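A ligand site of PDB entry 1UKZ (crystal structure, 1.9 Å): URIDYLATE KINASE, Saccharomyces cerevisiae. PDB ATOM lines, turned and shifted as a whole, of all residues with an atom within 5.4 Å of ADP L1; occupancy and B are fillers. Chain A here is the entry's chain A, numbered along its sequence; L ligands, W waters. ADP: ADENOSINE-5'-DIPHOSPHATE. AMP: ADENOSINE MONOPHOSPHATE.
The backbone NH of Ala 26 lies within hydrogen-bond range of an oxygen (O2B) of ADP L1 (3.2 Å).
An oxygen (O2B) of ADP L1 is in salt-bridge range of the side-chain amino group (NZ) of Lys 28 (2.7 Å).
An oxygen (O3B) of ADP L1 lies within hydrogen-bond range of the backbone NH of Gly 25 (2.8 Å).
The backbone NH (N) of Gly 27 lies within hydrogen-bond range of an oxygen (O2B) of ADP L1 (3.1 Å).
An oxygen (O1A) of ADP L1 lies within salt-bridge range of the guanidinium group (NH1) of Arg 141 (2.9 Å).
The side-chain hydroxyl (OG1) of Thr 30 lies within hydrogen-bond range of an oxygen (O2A) of ADP L1, at 2.6 Å.
The backbone NH (N) of Gly 29 is in hydrogen-bond range of an oxygen (O1B) of ADP L1, 2.9 Å away.
O1P of AMP L2 is in salt-bridge range of NH2 of Arg 158, 3.6 Å away.
O2B of ADP L1 sits at hydrogen-bond distance from N of Lys 28, 2.9 Å away.
The backbone carbonyl oxygen of Arg 186 sits at hydrogen-bond distance from a nitrogen (N6) of ADP L1 (2.8 Å).
The backbone NH (N) of Thr 30 lies within hydrogen-bond range of an oxygen (O2A) of ADP L1 (2.8 Å).
NH1 of Arg 137 is in hydrogen-bond range of O of Ala 26 (3.1 Å).
NH2 of Arg 137 is in hydrogen-bond range of O of Cys 184, at 2.7 Å.
The side-chain amino group (NZ) of Lys 28 sits at hydrogen-bond distance from the backbone carbonyl oxygen (O) of Gly 23, at 2.9 Å.
O of Val 188 lies close to OE1 of Gln 31, at 3.2 Å.
The guanidinium group (NH2) of Arg 137 sits close to a nitrogen (N6) of ADP L1, 3.4 Å away.
The backbone NH (N) of Val 188 sits close to a nitrogen (N6) of ADP L1 (3.5 Å).
Residues that only touch ADP L1: Ser 187 (3.7 Å), Gly 23 (3.8 Å), Pro 24 (3.8 Å) and Cys 184 (3.9 Å).
14 residues have an atom within 4 Å of ADP L1: Gly 23, Pro 24, Gly 25, Ala 26, Gly 27, Lys 28, Gly 29, Thr 30, Arg 137, Arg 141, Cys 184, Arg 186, Ser 187 and Val 188.
The nearest printed residue that does not touch ADP L1 is Val 191 (4.1 Å).
Water W10 lies within hydrogen-bond range of O1B of ADP L1 (2.6 Å) and OD1 of Asp 102 (2.8 Å).
Water W9 lies within hydrogen-bond range of an oxygen (O1P) of AMP L2, an oxygen (O3B) of ADP L1, the guanidinium group of Arg 141 and the guanidinium group of Arg 158.
Water W6 lies within hydrogen-bond range of N7 of ADP L1 (2.9 Å) and OE1 of Gln 31 (2.9 Å).
Water W8 lies within hydrogen-bond range of the side-chain hydroxyl (OG1) of Thr 30 and an oxygen (O2') of ADP L1.
Water W3 lies within hydrogen-bond range of O3P of AMP L2 (2.8 Å), NZ of Lys 28 (2.8 Å) and O3B of ADP L1 (3.1 Å).
Water W1 bridges a nitrogen (N1) of ADP L1 (3.1 Å) and the backbone carbonyl oxygen (O) of Arg 186 (3.3 Å).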
ATOM      1  N   GLY A  23     -10.914  17.901 -13.753  1.00  0.00           N
ATOM      2  CA  GLY A  23     -10.850  16.660 -14.487  1.00  0.00           C
ATOM      3  C   GLY A  23     -12.086  16.376 -15.292  1.00  0.00           C
ATOM      4  O   GLY A  23     -13.086  17.072 -15.143  1.00  0.00           O
ATOM      5  N   PRO A  24     -12.059  15.334 -16.136  1.00  0.00           N
ATOM      6  CA  PRO A  24     -13.222  14.993 -16.959  1.00  0.00           C
ATOM      7  C   PRO A  24     -14.397  14.555 -16.065  1.00  0.00           C
ATOM      8  O   PRO A  24     -14.201  13.782 -15.128  1.00  0.00           O
ATOM      9  CB  PRO A  24     -12.700  13.862 -17.840  1.00  0.00           C
ATOM     10  CG  PRO A  24     -11.676  13.181 -16.972  1.00  0.00           C
ATOM     11  CD  PRO A  24     -10.961  14.357 -16.313  1.00  0.00           C
ATOM     12  N   GLY A  25     -15.582  15.105 -16.338  1.00  0.00           N
ATOM     13  CA  GLY A  25     -16.769  14.758 -15.588  1.00  0.00           C
ATOM     14  C   GLY A  25     -16.923  15.497 -14.278  1.00  0.00           C
ATOM     15  O   GLY A  25     -17.747  15.127 -13.454  1.00  0.00           O
ATOM     16  N   ALA A  26     -16.123  16.544 -14.063  1.00  0.00           N
ATOM     17  CA  ALA A  26     -16.194  17.342 -12.844  1.00  0.00           C
ATOM     18  C   ALA A  26     -17.418  18.243 -12.863  1.00  0.00           C
ATOM     19  O   ALA A  26     -17.787  18.771 -11.820  1.00  0.00           O
ATOM     20  CB  ALA A  26     -14.933  18.193 -12.697  1.00  0.00           C
ATOM     21  N   GLY A  27     -17.989  18.460 -14.043  1.00  0.00           N
ATOM     22  CA  GLY A  27     -19.165  19.299 -14.184  1.00  0.00           C
ATOM     23  C   GLY A  27     -18.886  20.642 -14.847  1.00  0.00           C
ATOM     24  O   GLY A  27     -19.705  21.563 -14.781  1.00  0.00           O
ATOM     25  N   LYS A  28     -17.741  20.752 -15.519  1.00  0.00           N
ATOM     26  CA  LYS A  28     -17.358  22.008 -16.160  1.00  0.00           C
ATOM     27  C   LYS A  28     -18.343  22.461 -17.213  1.00  0.00           C
ATOM     28  O   LYS A  28     -18.858  23.580 -17.149  1.00  0.00           O
ATOM     29  CB  LYS A  28     -15.971  21.884 -16.779  1.00  0.00           C
ATOM     30  CG  LYS A  28     -14.880  21.563 -15.759  1.00  0.00           C
ATOM     31  CD  LYS A  28     -13.508  21.485 -16.398  1.00  0.00           C
ATOM     32  CE  LYS A  28     -13.498  20.526 -17.571  1.00  0.00           C
ATOM     33  NZ  LYS A  28     -13.711  19.127 -17.122  1.00  0.00           N
ATOM     34  N   GLY A  29     -18.643  21.569 -18.156  1.00  0.00           N
ATOM     35  CA  GLY A  29     -19.569  21.886 -19.211  1.00  0.00           C
ATOM     36  C   GLY A  29     -20.932  22.226 -18.658  1.00  0.00           C
ATOM     37  O   GLY A  29     -21.551  23.193 -19.075  1.00  0.00           O
ATOM     38  N   THR A  30     -21.393  21.429 -17.705  1.00  0.00           N
ATOM     39  CA  THR A  30     -22.684  21.647 -17.067  1.00  0.00           C
ATOM     40  C   THR A  30     -22.814  23.040 -16.449  1.00  0.00           C
ATOM     41  O   THR A  30     -23.772  23.775 -16.721  1.00  0.00           O
ATOM     42  CB  THR A  30     -22.943  20.572 -16.003  1.00  0.00           C
ATOM     43  OG1 THR A  30     -23.047  19.303 -16.647  1.00  0.00           O
ATOM     44  CG2 THR A  30     -24.235  20.871 -15.206  1.00  0.00           C
ATOM     45  N   GLN A  31     -21.818  23.426 -15.650  1.00  0.00           N
ATOM     46  CA  GLN A  31     -21.841  24.731 -14.985  1.00  0.00           C
ATOM     47  C   GLN A  31     -21.671  25.887 -15.937  1.00  0.00           C
ATOM     48  O   GLN A  31     -22.304  26.942 -15.768  1.00  0.00           O
ATOM     49  CB  GLN A  31     -20.788  24.793 -13.870  1.00  0.00           C
ATOM     50  CG  GLN A  31     -21.072  23.809 -12.717  1.00  0.00           C
ATOM     51  CD  GLN A  31     -22.418  24.067 -12.041  1.00  0.00           C
ATOM     52  OE1 GLN A  31     -23.145  23.127 -11.702  1.00  0.00           O
ATOM     53  NE2 GLN A  31     -22.737  25.314 -11.835  1.00  0.00           N
ATOM     54  N   ASP A 102     -13.575  26.485 -21.209  1.00  0.00           N
ATOM     55  CA  ASP A 102     -13.634  25.252 -20.470  1.00  0.00           C
ATOM     56  C   ASP A 102     -12.727  24.165 -21.059  1.00  0.00           C
ATOM     57  O   ASP A 102     -12.737  23.896 -22.252  1.00  0.00           O
ATOM     58  CB  ASP A 102     -15.145  24.925 -20.297  1.00  0.00           C
ATOM     59  CG  ASP A 102     -15.516  23.467 -20.528  1.00  0.00           C
ATOM     60  OD1 ASP A 102     -14.753  22.548 -20.238  1.00  0.00           O
ATOM     61  OD2 ASP A 102     -16.680  23.253 -20.952  1.00  0.00           O
ATOM     62  N   ARG A 137     -19.836   9.818 -12.771  1.00  0.00           N
ATOM     63  CA  ARG A 137     -20.498  10.750 -13.702  1.00  0.00           C
ATOM     64  C   ARG A 137     -20.177  10.438 -15.169  1.00  0.00           C
ATOM     65  O   ARG A 137     -21.037  10.568 -16.029  1.00  0.00           O
ATOM     66  CB  ARG A 137     -20.116  12.180 -13.396  1.00  0.00           C
ATOM     67  CG  ARG A 137     -20.742  12.673 -12.118  1.00  0.00           C
ATOM     68  CD  ARG A 137     -20.304  14.077 -11.849  1.00  0.00           C
ATOM     69  NE  ARG A 137     -20.733  14.514 -10.532  1.00  0.00           N
ATOM     70  CZ  ARG A 137     -20.361  15.662  -9.982  1.00  0.00           C
ATOM     71  NH1 ARG A 137     -19.564  16.482 -10.648  1.00  0.00           N
ATOM     72  NH2 ARG A 137     -20.782  15.969  -8.763  1.00  0.00           N
ATOM     73  N   LEU A 138     -18.941  10.036 -15.450  1.00  0.00           N
ATOM     74  CA  LEU A 138     -18.532   9.720 -16.813  1.00  0.00           C
ATOM     75  C   LEU A 138     -19.144   8.412 -17.301  1.00  0.00           C
ATOM     76  O   LEU A 138     -19.464   8.282 -18.482  1.00  0.00           O
ATOM     77  CB  LEU A 138     -17.013   9.663 -16.925  1.00  0.00           C
ATOM     78  CG  LEU A 138     -16.286  11.015 -16.841  1.00  0.00           C
ATOM     79  CD1 LEU A 138     -14.773  10.810 -16.867  1.00  0.00           C
ATOM     80  CD2 LEU A 138     -16.716  11.917 -17.964  1.00  0.00           C
ATOM     81  N   GLU A 140     -21.984   7.233 -16.275  1.00  0.00           N
ATOM     82  CA  GLU A 140     -23.382   7.583 -16.472  1.00  0.00           C
ATOM     83  C   GLU A 140     -23.517   8.362 -17.786  1.00  0.00           C
ATOM     84  O   GLU A 140     -24.431   8.107 -18.575  1.00  0.00           O
ATOM     85  CB  GLU A 140     -23.897   8.443 -15.314  1.00  0.00           C
ATOM     86  CG  GLU A 140     -24.620   7.642 -14.242  1.00  0.00           C
ATOM     87  CD  GLU A 140     -25.779   6.823 -14.801  1.00  0.00           C
ATOM     88  OE1 GLU A 140     -26.719   7.402 -15.407  1.00  0.00           O
ATOM     89  OE2 GLU A 140     -25.750   5.578 -14.641  1.00  0.00           O
ATOM     90  N   ARG A 141     -22.602   9.299 -18.022  1.00  0.00           N
ATOM     91  CA  ARG A 141     -22.606  10.096 -19.242  1.00  0.00           C
ATOM     92  C   ARG A 141     -22.363   9.225 -20.458  1.00  0.00           C
ATOM     93  O   ARG A 141     -22.948   9.442 -21.509  1.00  0.00           O
ATOM     94  CB  ARG A 141     -21.555  11.202 -19.186  1.00  0.00           C
ATOM     95  CG  ARG A 141     -21.787  12.293 -20.211  1.00  0.00           C
ATOM     96  CD  ARG A 141     -20.834  13.438 -20.038  1.00  0.00           C
ATOM     97  NE  ARG A 141     -19.512  13.091 -20.534  1.00  0.00           N
ATOM     98  CZ  ARG A 141     -18.435  13.861 -20.419  1.00  0.00           C
ATOM     99  NH1 ARG A 141     -18.516  15.042 -19.820  1.00  0.00           N
ATOM    100  NH2 ARG A 141     -17.279  13.434 -20.903  1.00  0.00           N
ATOM    101  N   ARG A 158      -7.664   9.378 -19.448  1.00  0.00           N
ATOM    102  CA  ARG A 158      -8.014  10.785 -19.225  1.00  0.00           C
ATOM    103  C   ARG A 158      -7.692  11.210 -17.780  1.00  0.00           C
ATOM    104  O   ARG A 158      -7.146  12.290 -17.568  1.00  0.00           O
ATOM    105  CB  ARG A 158      -9.496  11.020 -19.558  1.00  0.00           C
ATOM    106  CG  ARG A 158      -9.769  10.850 -21.044  1.00  0.00           C
ATOM    107  CD  ARG A 158     -11.203  10.500 -21.285  1.00  0.00           C
ATOM    108  NE  ARG A 158     -12.070  11.625 -20.981  1.00  0.00           N
ATOM    109  CZ  ARG A 158     -13.392  11.548 -20.943  1.00  0.00           C
ATOM    110  NH1 ARG A 158     -13.997  10.384 -21.177  1.00  0.00           N
ATOM    111  NH2 ARG A 158     -14.110  12.642 -20.786  1.00  0.00           N
ATOM    112  N   CYS A 184     -16.872  20.089  -6.636  1.00  0.00           N
ATOM    113  CA  CYS A 184     -17.736  19.510  -7.660  1.00  0.00           C
ATOM    114  C   CYS A 184     -18.789  18.559  -7.101  1.00  0.00           C
ATOM    115  O   CYS A 184     -19.812  18.306  -7.721  1.00  0.00           O
ATOM    116  CB  CYS A 184     -16.874  18.674  -8.581  1.00  0.00           C
ATOM    117  SG  CYS A 184     -16.614  17.034  -7.817  1.00  0.00           S
ATOM    118  N   ARG A 186     -21.432  18.133  -5.268  1.00  0.00           N
ATOM    119  CA  ARG A 186     -22.699  18.551  -4.673  1.00  0.00           C
ATOM    120  C   ARG A 186     -23.684  18.518  -5.830  1.00  0.00           C
ATOM    121  O   ARG A 186     -23.327  18.155  -6.947  1.00  0.00           O
ATOM    122  CB  ARG A 186     -22.563  19.938  -4.035  1.00  0.00           C
ATOM    123  CG  ARG A 186     -21.897  19.888  -2.665  1.00  0.00           C
ATOM    124  CD  ARG A 186     -21.465  21.262  -2.183  1.00  0.00           C
ATOM    125  NE  ARG A 186     -20.421  21.808  -3.057  1.00  0.00           N
ATOM    126  CZ  ARG A 186     -20.510  22.973  -3.684  1.00  0.00           C
ATOM    127  NH1 ARG A 186     -21.591  23.729  -3.533  1.00  0.00           N
ATOM    128  NH2 ARG A 186     -19.537  23.387  -4.483  1.00  0.00           N
ATOM    129  N   SER A 187     -24.954  18.812  -5.579  1.00  0.00           N
ATOM    130  CA  SER A 187     -25.927  18.801  -6.661  1.00  0.00           C
ATOM    131  C   SER A 187     -25.567  19.941  -7.623  1.00  0.00           C
ATOM    132  O   SER A 187     -24.844  20.880  -7.257  1.00  0.00           O
ATOM    133  CB  SER A 187     -27.338  19.014  -6.135  1.00  0.00           C
ATOM    134  OG  SER A 187     -27.447  20.241  -5.426  1.00  0.00           O
ATOM    135  N   VAL A 188     -26.080  19.846  -8.841  1.00  0.00           N
ATOM    136  CA  VAL A 188     -25.836  20.854  -9.856  1.00  0.00           C
ATOM    137  C   VAL A 188     -26.191  22.230  -9.293  1.00  0.00           C
ATOM    138  O   VAL A 188     -25.397  23.167  -9.413  1.00  0.00           O
ATOM    139  CB  VAL A 188     -26.691  20.584 -11.113  1.00  0.00           C
ATOM    140  CG1 VAL A 188     -26.562  21.726 -12.100  1.00  0.00           C
ATOM    141  CG2 VAL A 188     -26.272  19.276 -11.743  1.00  0.00           C
ATOM    142  N   VAL A 191     -23.738  23.348  -6.482  1.00  0.00           N
ATOM    143  CA  VAL A 191     -22.444  23.717  -7.048  1.00  0.00           C
ATOM    144  C   VAL A 191     -22.561  25.075  -7.712  1.00  0.00           C
ATOM    145  O   VAL A 191     -21.712  25.948  -7.551  1.00  0.00           O
ATOM    146  CB  VAL A 191     -21.975  22.705  -8.094  1.00  0.00           C
ATOM    147  CG1 VAL A 191     -20.702  23.199  -8.763  1.00  0.00           C
ATOM    148  CG2 VAL A 191     -21.750  21.386  -7.451  1.00  0.00           C
HETATM  149  PB  ADP L   1     -17.075  18.009 -17.661  1.00  0.00           P
HETATM  150  O1B ADP L   1     -17.416  18.970 -18.678  1.00  0.00           O
HETATM  151  O2B ADP L   1     -16.247  18.490 -16.600  1.00  0.00           O
HETATM  152  O3B ADP L   1     -16.369  16.854 -18.350  1.00  0.00           O
HETATM  153  PA  ADP L   1     -19.981  17.504 -17.319  1.00  0.00           P
HETATM  154  O1A ADP L   1     -20.297  16.928 -18.567  1.00  0.00           O
HETATM  155  O2A ADP L   1     -20.514  18.814 -17.105  1.00  0.00           O
HETATM  156  O3A ADP L   1     -18.429  17.471 -17.140  1.00  0.00           O
HETATM  157  O5' ADP L   1     -20.550  16.588 -16.220  1.00  0.00           O
HETATM  158  C5' ADP L   1     -20.257  15.183 -16.292  1.00  0.00           C
HETATM  159  C4' ADP L   1     -21.516  14.328 -16.279  1.00  0.00           C
HETATM  160  O4' ADP L   1     -22.094  14.355 -14.965  1.00  0.00           O
HETATM  161  C3' ADP L   1     -22.663  14.767 -17.250  1.00  0.00           C
HETATM  162  O3' ADP L   1     -23.467  13.654 -17.535  1.00  0.00           O
HETATM  163  C2' ADP L   1     -23.430  15.805 -16.424  1.00  0.00           C
HETATM  164  O2' ADP L   1     -24.857  15.803 -16.648  1.00  0.00           O
HETATM  165  C1' ADP L   1     -23.042  15.422 -14.991  1.00  0.00           C
HETATM  166  N9  ADP L   1     -23.169  16.293 -13.883  1.00  0.00           N
HETATM  167  C8  ADP L   1     -22.602  17.518 -13.933  1.00  0.00           C
HETATM  168  N7  ADP L   1     -22.576  18.058 -12.775  1.00  0.00           N
HETATM  169  C5  ADP L   1     -23.156  17.209 -11.888  1.00  0.00           C
HETATM  170  C6  ADP L   1     -23.434  17.280 -10.512  1.00  0.00           C
HETATM  171  N6  ADP L   1     -23.083  18.309  -9.767  1.00  0.00           N
HETATM  172  N1  ADP L   1     -24.070  16.229  -9.986  1.00  0.00           N
HETATM  173  C2  ADP L   1     -24.414  15.177 -10.737  1.00  0.00           C
HETATM  174  N3  ADP L   1     -24.205  14.988 -12.038  1.00  0.00           N
HETATM  175  C4  ADP L   1     -23.570  16.064 -12.598  1.00  0.00           C
HETATM  176  P   AMP L   2     -13.276  17.059 -23.005  1.00  0.00           P
HETATM  177  O1P AMP L   2     -13.334  15.895 -22.037  1.00  0.00           O
HETATM  178  O2P AMP L   2     -14.442  17.051 -23.794  1.00  0.00           O
HETATM  179  O3P AMP L   2     -12.987  18.281 -22.340  1.00  0.00           O
HETATM  180  O5' AMP L   2     -12.020  16.700 -23.903  1.00  0.00           O
HETATM  181  C5' AMP L   2     -11.987  15.534 -24.721  1.00  0.00           C
HETATM  182  C4' AMP L   2     -10.613  15.181 -25.223  1.00  0.00           C
HETATM  183  O4' AMP L   2     -10.164  16.173 -26.171  1.00  0.00           O
HETATM  184  C3' AMP L   2      -9.554  15.220 -24.082  1.00  0.00           C
HETATM  185  O3' AMP L   2      -9.477  14.018 -23.326  1.00  0.00           O
HETATM  186  C2' AMP L   2      -8.243  15.410 -24.868  1.00  0.00           C
HETATM  187  O2' AMP L   2      -7.973  14.229 -25.602  1.00  0.00           O
HETATM  188  C1' AMP L   2      -8.921  16.556 -25.658  1.00  0.00           C
HETATM  189  N9  AMP L   2      -8.625  17.904 -25.354  1.00  0.00           N
HETATM  190  C8  AMP L   2      -9.540  18.588 -24.622  1.00  0.00           C
HETATM  191  N7  AMP L   2      -9.056  19.721 -24.250  1.00  0.00           N
HETATM  192  C5  AMP L   2      -7.777  19.837 -24.734  1.00  0.00           C
HETATM  193  C6  AMP L   2      -6.815  20.828 -24.624  1.00  0.00           C
HETATM  194  N6  AMP L   2      -7.025  21.915 -23.880  1.00  0.00           N
HETATM  195  N1  AMP L   2      -5.648  20.612 -25.273  1.00  0.00           N
HETATM  196  C2  AMP L   2      -5.458  19.487 -25.948  1.00  0.00           C
HETATM  197  N3  AMP L   2      -6.282  18.440 -26.119  1.00  0.00           N
HETATM  198  C4  AMP L   2      -7.479  18.660 -25.475  1.00  0.00           C
HETATM  199  O   HOH W   1     -24.846  15.279  -7.095  1.00  0.00           O
HETATM  200  O   HOH W   2     -18.854  18.545 -21.089  1.00  0.00           O
HETATM  201  O   HOH W   3     -13.869  17.979 -19.711  1.00  0.00           O
HETATM  202  O   HOH W   4     -23.780  11.633 -15.741  1.00  0.00           O
HETATM  203  O   HOH W   5     -24.583  14.298 -20.268  1.00  0.00           O
HETATM  204  O   HOH W   6     -21.972  20.486 -11.363  1.00  0.00           O
HETATM  205  O   HOH W   7     -24.484  12.206 -13.079  1.00  0.00           O
HETATM  206  O   HOH W   8     -25.079  18.293 -18.245  1.00  0.00           O
HETATM  207  O   HOH W   9     -15.131  15.404 -20.219  1.00  0.00           O
HETATM  208  O   HOH W  10     -15.814  20.005 -20.464  1.00  0.00           O
